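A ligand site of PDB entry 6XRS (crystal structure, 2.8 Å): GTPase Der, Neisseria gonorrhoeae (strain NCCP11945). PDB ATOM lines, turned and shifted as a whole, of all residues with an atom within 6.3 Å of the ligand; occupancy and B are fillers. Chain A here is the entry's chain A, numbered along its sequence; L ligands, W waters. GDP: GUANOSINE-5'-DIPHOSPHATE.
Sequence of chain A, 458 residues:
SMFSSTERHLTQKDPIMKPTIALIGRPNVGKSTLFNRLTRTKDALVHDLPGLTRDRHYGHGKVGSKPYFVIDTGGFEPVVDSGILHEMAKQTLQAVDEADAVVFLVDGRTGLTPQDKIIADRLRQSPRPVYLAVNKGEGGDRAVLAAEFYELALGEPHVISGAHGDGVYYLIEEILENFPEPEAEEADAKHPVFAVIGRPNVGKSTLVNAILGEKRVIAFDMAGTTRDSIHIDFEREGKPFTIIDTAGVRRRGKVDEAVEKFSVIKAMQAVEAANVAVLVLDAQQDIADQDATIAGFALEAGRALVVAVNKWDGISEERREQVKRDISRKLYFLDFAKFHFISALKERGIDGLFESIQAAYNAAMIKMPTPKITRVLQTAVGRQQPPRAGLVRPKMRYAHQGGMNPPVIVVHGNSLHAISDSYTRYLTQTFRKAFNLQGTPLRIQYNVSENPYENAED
An oxygen (O1B) of the ligand lies within hydrogen-bond range of the backbone NH (N) of Lys 204 (2.6 Å).
The side-chain amino group of Lys 204 is in salt-bridge range of an oxygen (O1B) of the ligand.
An oxygen (O1A) of the ligand sits at hydrogen-bond distance from the backbone NH of Thr 206.
The side-chain hydroxyl (OG1) of Thr 206 lies within hydrogen-bond range of an oxygen (O1A) of the ligand (2.7 Å).
A nitrogen (N1) of the ligand lies within hydrogen-bond range of the side-chain carboxylate (OD1) of Asp 313 (2.8 Å).
An oxygen (O2B) of the ligand sits at hydrogen-bond distance from the backbone NH (N) of Asn 201 (2.8 Å).
N of Ser 205 lies within hydrogen-bond range of O3B of the ligand (2.8 Å).
The side-chain hydroxyl (OG) of Ser 205 is in hydrogen-bond range of an oxygen (O3B) of the ligand (3.0 Å).
An oxygen (O6) of the ligand sits at hydrogen-bond distance from the backbone NH (N) of Leu 345, 3.0 Å away.
The backbone NH of Gly 203 is in hydrogen-bond range of an oxygen (O1B) of the ligand (3.0 Å).
N of Ala 344 sits at hydrogen-bond distance from O6 of the ligand (3.0 Å).
The side-chain hydroxyl of Ser 343 lies within hydrogen-bond range of an oxygen (O6) of the ligand.
ND2 of Asn 310 is in hydrogen-bond range of N7 of the ligand, 3.4 Å away.
The backbone NH (N) of Val 202 is in hydrogen-bond range of an oxygen (O1B) of the ligand.
The backbone carbonyl oxygen (O) of Arg 199 sits at hydrogen-bond distance from the side-chain amino group (NZ) of Lys 204, at 2.9 Å.
The backbone carbonyl oxygen (O) of Gly 198 sits at hydrogen-bond distance from the side-chain amino group (NZ) of Lys 204 (3.1 Å).
The side-chain hydroxyl (OG) of Ser 343 sits at hydrogen-bond distance from the side-chain carboxylate (OD1) of Asp 313 (2.8 Å).
NZ of Lys 311 sits at hydrogen-bond distance from O of Asn 201, 2.8 Å away.
The side-chain amide oxygen (OD1) of Asn 310 is in hydrogen-bond range of the backbone NH (N) of Ala 344 (2.8 Å).
The side-chain hydroxyl (OG) of Ser 343 lies within hydrogen-bond range of the backbone NH (N) of Lys 346.
The side-chain amide oxygen (OD1) of Asn 310 lies close to the backbone carbonyl oxygen (O) of Ile 342 (3.5 Å).
The backbone NH (N) of Lys 311 is in hydrogen-bond range of the backbone carbonyl oxygen (O) of Ile 342 (3.3 Å).
Pro 200 touches the ligand.
Lys 311 touches the ligand (NZ to O4', 3.5 Å).
Hydrophobic or aromatic side chains that line the ligand: Val 202 and Leu 345.
Water W1 lies within hydrogen-bond range of the side-chain amino group of Lys 204 (3.1 Å) and an oxygen (O2B) of the ligand (3.3 Å).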
ATOM      1  N   GLY A 198     -31.900  -5.683  -3.747  1.00  0.00           N
ATOM      2  CA  GLY A 198     -31.425  -6.517  -4.826  1.00  0.00           C
ATOM      3  C   GLY A 198     -31.746  -7.975  -4.609  1.00  0.00           C
ATOM      4  O   GLY A 198     -32.080  -8.421  -3.517  1.00  0.00           O
ATOM      5  N   ARG A 199     -31.573  -8.737  -5.685  1.00  0.00           N
ATOM      6  CA  ARG A 199     -31.844 -10.171  -5.774  1.00  0.00           C
ATOM      7  C   ARG A 199     -31.164 -10.954  -4.659  1.00  0.00           C
ATOM      8  O   ARG A 199     -30.162 -10.500  -4.112  1.00  0.00           O
ATOM      9  CB  ARG A 199     -31.289 -10.684  -7.088  1.00  0.00           C
ATOM     10  CG  ARG A 199     -32.221 -10.804  -8.244  1.00  0.00           C
ATOM     11  CD  ARG A 199     -31.555 -11.767  -9.208  1.00  0.00           C
ATOM     12  NE  ARG A 199     -30.182 -11.381  -9.535  1.00  0.00           N
ATOM     13  CZ  ARG A 199     -29.243 -12.243  -9.938  1.00  0.00           C
ATOM     14  NH1 ARG A 199     -29.538 -13.521 -10.047  1.00  0.00           N
ATOM     15  NH2 ARG A 199     -28.017 -11.826 -10.227  1.00  0.00           N
ATOM     16  N   PRO A 200     -31.621 -12.159  -4.336  1.00  0.00           N
ATOM     17  CA  PRO A 200     -30.854 -12.988  -3.405  1.00  0.00           C
ATOM     18  C   PRO A 200     -29.451 -13.212  -3.920  1.00  0.00           C
ATOM     19  O   PRO A 200     -29.235 -13.344  -5.133  1.00  0.00           O
ATOM     20  CB  PRO A 200     -31.648 -14.300  -3.372  1.00  0.00           C
ATOM     21  CG  PRO A 200     -33.027 -13.912  -3.758  1.00  0.00           C
ATOM     22  CD  PRO A 200     -32.872 -12.808  -4.753  1.00  0.00           C
ATOM     23  N   ASN A 201     -28.478 -13.207  -3.015  1.00  0.00           N
ATOM     24  CA  ASN A 201     -27.123 -13.692  -3.243  1.00  0.00           C
ATOM     25  C   ASN A 201     -26.243 -12.750  -4.065  1.00  0.00           C
ATOM     26  O   ASN A 201     -25.180 -13.163  -4.543  1.00  0.00           O
ATOM     27  CB  ASN A 201     -27.149 -15.092  -3.864  1.00  0.00           C
ATOM     28  CG  ASN A 201     -26.959 -16.190  -2.825  1.00  0.00           C
ATOM     29  OD1 ASN A 201     -25.815 -16.520  -2.464  1.00  0.00           O
ATOM     30  ND2 ASN A 201     -28.072 -16.721  -2.298  1.00  0.00           N
ATOM     31  N   VAL A 202     -26.638 -11.496  -4.229  1.00  0.00           N
ATOM     32  CA  VAL A 202     -25.797 -10.559  -4.957  1.00  0.00           C
ATOM     33  C   VAL A 202     -24.764  -9.872  -4.071  1.00  0.00           C
ATOM     34  O   VAL A 202     -23.822  -9.256  -4.601  1.00  0.00           O
ATOM     35  CB  VAL A 202     -26.664  -9.507  -5.671  1.00  0.00           C
ATOM     36  CG1 VAL A 202     -27.636 -10.201  -6.591  1.00  0.00           C
ATOM     37  CG2 VAL A 202     -27.434  -8.663  -4.628  1.00  0.00           C
ATOM     38  N   GLY A 203     -24.914  -9.931  -2.751  1.00  0.00           N
ATOM     39  CA  GLY A 203     -23.901  -9.377  -1.871  1.00  0.00           C
ATOM     40  C   GLY A 203     -24.394  -8.303  -0.935  1.00  0.00           C
ATOM     41  O   GLY A 203     -23.592  -7.530  -0.388  1.00  0.00           O
ATOM     42  N   LYS A 204     -25.719  -8.234  -0.742  1.00  0.00           N
ATOM     43  CA  LYS A 204     -26.304  -7.196   0.111  1.00  0.00           C
ATOM     44  C   LYS A 204     -25.783  -7.288   1.540  1.00  0.00           C
ATOM     45  O   LYS A 204     -25.376  -6.277   2.111  1.00  0.00           O
ATOM     46  CB  LYS A 204     -27.824  -7.294   0.086  1.00  0.00           C
ATOM     47  CG  LYS A 204     -28.348  -7.193  -1.303  1.00  0.00           C
ATOM     48  CD  LYS A 204     -29.845  -7.141  -1.369  1.00  0.00           C
ATOM     49  CE  LYS A 204     -30.452  -8.360  -0.750  1.00  0.00           C
ATOM     50  NZ  LYS A 204     -30.113  -9.611  -1.402  1.00  0.00           N
ATOM     51  N   SER A 205     -25.778  -8.496   2.124  1.00  0.00           N
ATOM     52  CA  SER A 205     -25.260  -8.610   3.493  1.00  0.00           C
ATOM     53  C   SER A 205     -23.782  -8.243   3.543  1.00  0.00           C
ATOM     54  O   SER A 205     -23.356  -7.477   4.415  1.00  0.00           O
ATOM     55  CB  SER A 205     -25.461 -10.004   4.070  1.00  0.00           C
ATOM     56  OG  SER A 205     -26.830 -10.301   4.175  1.00  0.00           O
ATOM     57  N   THR A 206     -22.991  -8.748   2.598  1.00  0.00           N
ATOM     58  CA  THR A 206     -21.574  -8.419   2.586  1.00  0.00           C
ATOM     59  C   THR A 206     -21.383  -6.916   2.408  1.00  0.00           C
ATOM     60  O   THR A 206     -20.508  -6.322   3.053  1.00  0.00           O
ATOM     61  CB  THR A 206     -20.866  -9.191   1.484  1.00  0.00           C
ATOM     62  OG1 THR A 206     -21.357 -10.533   1.474  1.00  0.00           O
ATOM     63  CG2 THR A 206     -19.369  -9.188   1.709  1.00  0.00           C
ATOM     64  N   LEU A 207     -22.183  -6.294   1.551  1.00  0.00           N
ATOM     65  CA  LEU A 207     -22.054  -4.856   1.349  1.00  0.00           C
ATOM     66  C   LEU A 207     -22.415  -4.068   2.619  1.00  0.00           C
ATOM     67  O   LEU A 207     -21.724  -3.104   2.974  1.00  0.00           O
ATOM     68  CB  LEU A 207     -22.916  -4.420   0.168  1.00  0.00           C
ATOM     69  CG  LEU A 207     -22.853  -2.904  -0.101  1.00  0.00           C
ATOM     70  CD1 LEU A 207     -21.407  -2.495  -0.285  1.00  0.00           C
ATOM     71  CD2 LEU A 207     -23.697  -2.494  -1.300  1.00  0.00           C
ATOM     72  N   LYS A 261     -34.835 -15.644   3.865  1.00  0.00           N
ATOM     73  CA  LYS A 261     -34.071 -14.395   3.875  1.00  0.00           C
ATOM     74  C   LYS A 261     -34.749 -13.323   3.003  1.00  0.00           C
ATOM     75  O   LYS A 261     -35.262 -12.338   3.532  1.00  0.00           O
ATOM     76  CB  LYS A 261     -32.632 -14.639   3.391  1.00  0.00           C
ATOM     77  N   VAL A 280     -28.011  -3.531  -5.663  1.00  0.00           N
ATOM     78  CA  VAL A 280     -26.805  -4.351  -5.795  1.00  0.00           C
ATOM     79  C   VAL A 280     -27.028  -5.401  -6.874  1.00  0.00           C
ATOM     80  O   VAL A 280     -28.031  -6.117  -6.875  1.00  0.00           O
ATOM     81  CB  VAL A 280     -26.439  -5.013  -4.455  1.00  0.00           C
ATOM     82  CG1 VAL A 280     -25.192  -5.860  -4.578  1.00  0.00           C
ATOM     83  CG2 VAL A 280     -26.259  -3.954  -3.397  1.00  0.00           C
ATOM     84  N   GLN A 284     -21.262 -11.225 -11.850  1.00  0.00           N
ATOM     85  CA  GLN A 284     -20.841 -12.511 -12.382  1.00  0.00           C
ATOM     86  C   GLN A 284     -21.970 -13.277 -13.033  1.00  0.00           C
ATOM     87  O   GLN A 284     -21.765 -14.431 -13.413  1.00  0.00           O
ATOM     88  CB  GLN A 284     -20.203 -13.340 -11.274  1.00  0.00           C
ATOM     89  CG  GLN A 284     -18.835 -12.826 -10.842  1.00  0.00           C
ATOM     90  CD  GLN A 284     -18.269 -13.576  -9.651  1.00  0.00           C
ATOM     91  OE1 GLN A 284     -17.058 -13.586  -9.415  1.00  0.00           O
ATOM     92  NE2 GLN A 284     -19.166 -14.168  -8.856  1.00  0.00           N
ATOM     93  N   ASN A 310     -21.719  -5.342  -8.140  1.00  0.00           N
ATOM     94  CA  ASN A 310     -20.889  -6.001  -7.145  1.00  0.00           C
ATOM     95  C   ASN A 310     -20.190  -7.234  -7.739  1.00  0.00           C
ATOM     96  O   ASN A 310     -20.480  -7.669  -8.860  1.00  0.00           O
ATOM     97  CB  ASN A 310     -21.742  -6.362  -5.935  1.00  0.00           C
ATOM     98  CG  ASN A 310     -20.906  -6.771  -4.729  1.00  0.00           C
ATOM     99  OD1 ASN A 310     -19.840  -6.227  -4.487  1.00  0.00           O
ATOM    100  ND2 ASN A 310     -21.426  -7.715  -3.951  1.00  0.00           N
ATOM    101  N   LYS A 311     -19.241  -7.773  -6.961  1.00  0.00           N
ATOM    102  CA  LYS A 311     -18.412  -8.923  -7.345  1.00  0.00           C
ATOM    103  C   LYS A 311     -17.540  -8.616  -8.568  1.00  0.00           C
ATOM    104  O   LYS A 311     -17.238  -9.504  -9.368  1.00  0.00           O
ATOM    105  CB  LYS A 311     -19.275 -10.162  -7.599  1.00  0.00           C
ATOM    106  CG  LYS A 311     -20.166 -10.534  -6.429  1.00  0.00           C
ATOM    107  CD  LYS A 311     -20.845 -11.888  -6.596  1.00  0.00           C
ATOM    108  CE  LYS A 311     -21.902 -12.058  -5.514  1.00  0.00           C
ATOM    109  NZ  LYS A 311     -22.693 -13.298  -5.715  1.00  0.00           N
ATOM    110  N   TRP A 312     -17.138  -7.352  -8.719  1.00  0.00           N
ATOM    111  CA  TRP A 312     -16.288  -6.948  -9.820  1.00  0.00           C
ATOM    112  C   TRP A 312     -14.933  -7.624  -9.735  1.00  0.00           C
ATOM    113  O   TRP A 312     -14.241  -7.753 -10.749  1.00  0.00           O
ATOM    114  CB  TRP A 312     -16.172  -5.420  -9.811  1.00  0.00           C
ATOM    115  CG  TRP A 312     -15.835  -4.769 -11.105  1.00  0.00           C
ATOM    116  CD1 TRP A 312     -14.777  -3.947 -11.347  1.00  0.00           C
ATOM    117  CD2 TRP A 312     -16.578  -4.850 -12.315  1.00  0.00           C
ATOM    118  NE1 TRP A 312     -14.802  -3.515 -12.654  1.00  0.00           N
ATOM    119  CE2 TRP A 312     -15.902  -4.058 -13.263  1.00  0.00           C
ATOM    120  CE3 TRP A 312     -17.740  -5.513 -12.702  1.00  0.00           C
ATOM    121  CZ2 TRP A 312     -16.357  -3.916 -14.580  1.00  0.00           C
ATOM    122  CZ3 TRP A 312     -18.188  -5.372 -13.996  1.00  0.00           C
ATOM    123  CH2 TRP A 312     -17.498  -4.582 -14.927  1.00  0.00           C
ATOM    124  N   ASP A 313     -14.576  -8.098  -8.544  1.00  0.00           N
ATOM    125  CA  ASP A 313     -13.316  -8.804  -8.345  1.00  0.00           C
ATOM    126  C   ASP A 313     -13.237 -10.067  -9.205  1.00  0.00           C
ATOM    127  O   ASP A 313     -12.141 -10.500  -9.562  1.00  0.00           O
ATOM    128  CB  ASP A 313     -13.154  -9.187  -6.875  1.00  0.00           C
ATOM    129  CG  ASP A 313     -14.406  -9.899  -6.310  1.00  0.00           C
ATOM    130  OD1 ASP A 313     -15.436  -9.220  -6.078  1.00  0.00           O
ATOM    131  OD2 ASP A 313     -14.380 -11.141  -6.145  1.00  0.00           O
ATOM    132  N   GLY A 314     -14.389 -10.639  -9.556  1.00  0.00           N
ATOM    133  CA  GLY A 314     -14.388 -11.863 -10.346  1.00  0.00           C
ATOM    134  C   GLY A 314     -14.174 -11.649 -11.832  1.00  0.00           C
ATOM    135  O   GLY A 314     -13.679 -12.549 -12.513  1.00  0.00           O
ATOM    136  N   ILE A 342     -17.835  -2.401  -7.855  1.00  0.00           N
ATOM    137  CA  ILE A 342     -17.249  -2.556  -6.537  1.00  0.00           C
ATOM    138  C   ILE A 342     -17.071  -4.034  -6.214  1.00  0.00           C
ATOM    139  O   ILE A 342     -17.648  -4.905  -6.863  1.00  0.00           O
ATOM    140  CB  ILE A 342     -18.111  -1.880  -5.435  1.00  0.00           C
ATOM    141  CG1 ILE A 342     -19.359  -2.717  -5.163  1.00  0.00           C
ATOM    142  CG2 ILE A 342     -18.511  -0.466  -5.832  1.00  0.00           C
ATOM    143  CD1 ILE A 342     -20.145  -2.244  -3.969  1.00  0.00           C
ATOM    144  N   SER A 343     -16.310  -4.300  -5.162  1.00  0.00           N
ATOM    145  CA  SER A 343     -16.215  -5.650  -4.593  1.00  0.00           C
ATOM    146  C   SER A 343     -16.495  -5.526  -3.096  1.00  0.00           C
ATOM    147  O   SER A 343     -15.632  -5.070  -2.336  1.00  0.00           O
ATOM    148  CB  SER A 343     -14.859  -6.278  -4.862  1.00  0.00           C
ATOM    149  OG  SER A 343     -14.715  -7.459  -4.090  1.00  0.00           O
ATOM    150  N   ALA A 344     -17.704  -5.918  -2.684  1.00  0.00           N
ATOM    151  CA  ALA A 344     -18.044  -5.901  -1.261  1.00  0.00           C
ATOM    152  C   ALA A 344     -17.140  -6.827  -0.457  1.00  0.00           C
ATOM    153  O   ALA A 344     -16.722  -6.497   0.653  1.00  0.00           O
ATOM    154  CB  ALA A 344     -19.508  -6.283  -1.057  1.00  0.00           C
ATOM    155  N   LEU A 345     -16.819  -7.992  -1.027  1.00  0.00           N
ATOM    156  CA  LEU A 345     -15.990  -8.954  -0.302  1.00  0.00           C
ATOM    157  C   LEU A 345     -14.629  -8.361   0.009  1.00  0.00           C
ATOM    158  O   LEU A 345     -14.238  -8.244   1.171  1.00  0.00           O
ATOM    159  CB  LEU A 345     -15.873 -10.247  -1.110  1.00  0.00           C
ATOM    160  CG  LEU A 345     -15.191 -11.434  -0.407  1.00  0.00           C
ATOM    161  CD1 LEU A 345     -15.886 -11.741   0.898  1.00  0.00           C
ATOM    162  CD2 LEU A 345     -15.259 -12.657  -1.309  1.00  0.00           C
ATOM    163  N   LYS A 346     -13.908  -7.934  -1.030  1.00  0.00           N
ATOM    164  CA  LYS A 346     -12.581  -7.353  -0.850  1.00  0.00           C
ATOM    165  C   LYS A 346     -12.666  -5.891  -0.436  1.00  0.00           C
ATOM    166  O   LYS A 346     -11.612  -5.235  -0.300  1.00  0.00           O
ATOM    167  CB  LYS A 346     -11.770  -7.508  -2.140  1.00  0.00           C
ATOM    168  N   GLU A 347     -13.882  -5.365  -0.228  1.00  0.00           N
ATOM    169  CA  GLU A 347     -14.108  -4.037   0.349  1.00  0.00           C
ATOM    170  C   GLU A 347     -13.383  -2.967  -0.454  1.00  0.00           C
ATOM    171  O   GLU A 347     -12.733  -2.075   0.104  1.00  0.00           O
ATOM    172  CB  GLU A 347     -13.724  -3.995   1.819  1.00  0.00           C
ATOM    173  CG  GLU A 347     -14.412  -5.068   2.666  1.00  0.00           C
ATOM    174  CD  GLU A 347     -14.275  -4.843   4.175  1.00  0.00           C
ATOM    175  OE1 GLU A 347     -14.417  -3.688   4.644  1.00  0.00           O
ATOM    176  OE2 GLU A 347     -13.969  -5.834   4.887  1.00  0.00           O
HETATM  177  PB  GDP L   1     -27.152 -11.334  -0.176  1.00  0.00           P
HETATM  178  O1B GDP L   1     -27.433 -10.203  -1.142  1.00  0.00           O
HETATM  179  O2B GDP L   1     -28.241 -12.366  -0.386  1.00  0.00           O
HETATM  180  O3B GDP L   1     -27.121 -10.790   1.240  1.00  0.00           O
HETATM  181  O3A GDP L   1     -25.696 -11.937  -0.552  1.00  0.00           O
HETATM  182  PA  GDP L   1     -24.577 -12.258   0.559  1.00  0.00           P
HETATM  183  O1A GDP L   1     -24.000 -10.995   1.173  1.00  0.00           O
HETATM  184  O2A GDP L   1     -25.195 -13.157   1.600  1.00  0.00           O
HETATM  185  O5' GDP L   1     -23.480 -13.036  -0.320  1.00  0.00           O
HETATM  186  C5' GDP L   1     -23.779 -14.333  -0.819  1.00  0.00           C
HETATM  187  C4' GDP L   1     -22.517 -14.920  -1.442  1.00  0.00           C
HETATM  188  O4' GDP L   1     -21.961 -13.966  -2.352  1.00  0.00           O
HETATM  189  C3' GDP L   1     -21.468 -15.227  -0.387  1.00  0.00           C
HETATM  190  O3' GDP L   1     -20.936 -16.552  -0.591  1.00  0.00           O
HETATM  191  C2' GDP L   1     -20.407 -14.173  -0.635  1.00  0.00           C
HETATM  192  O2' GDP L   1     -19.108 -14.709  -0.370  1.00  0.00           O
HETATM  193  C1' GDP L   1     -20.580 -13.766  -2.093  1.00  0.00           C
HETATM  194  N9  GDP L   1     -20.112 -12.365  -2.310  1.00  0.00           N
HETATM  195  C8  GDP L   1     -20.601 -11.226  -1.776  1.00  0.00           C
HETATM  196  N7  GDP L   1     -19.893 -10.131  -2.199  1.00  0.00           N
HETATM  197  C5  GDP L   1     -18.935 -10.566  -3.014  1.00  0.00           C
HETATM  198  C6  GDP L   1     -17.837  -9.965  -3.809  1.00  0.00           C
HETATM  199  O6  GDP L   1     -17.626  -8.725  -3.820  1.00  0.00           O
HETATM  200  N1  GDP L   1     -17.073 -10.797  -4.518  1.00  0.00           N
HETATM  201  C2  GDP L   1     -17.265 -12.132  -4.539  1.00  0.00           C
HETATM  202  N2  GDP L   1     -16.452 -12.911  -5.297  1.00  0.00           N
HETATM  203  N3  GDP L   1     -18.234 -12.742  -3.840  1.00  0.00           N
HETATM  204  C4  GDP L   1     -19.085 -12.028  -3.078  1.00  0.00           C
HETATM  205  O   HOH W   1     -31.402 -11.802   0.373  1.00  0.00           O
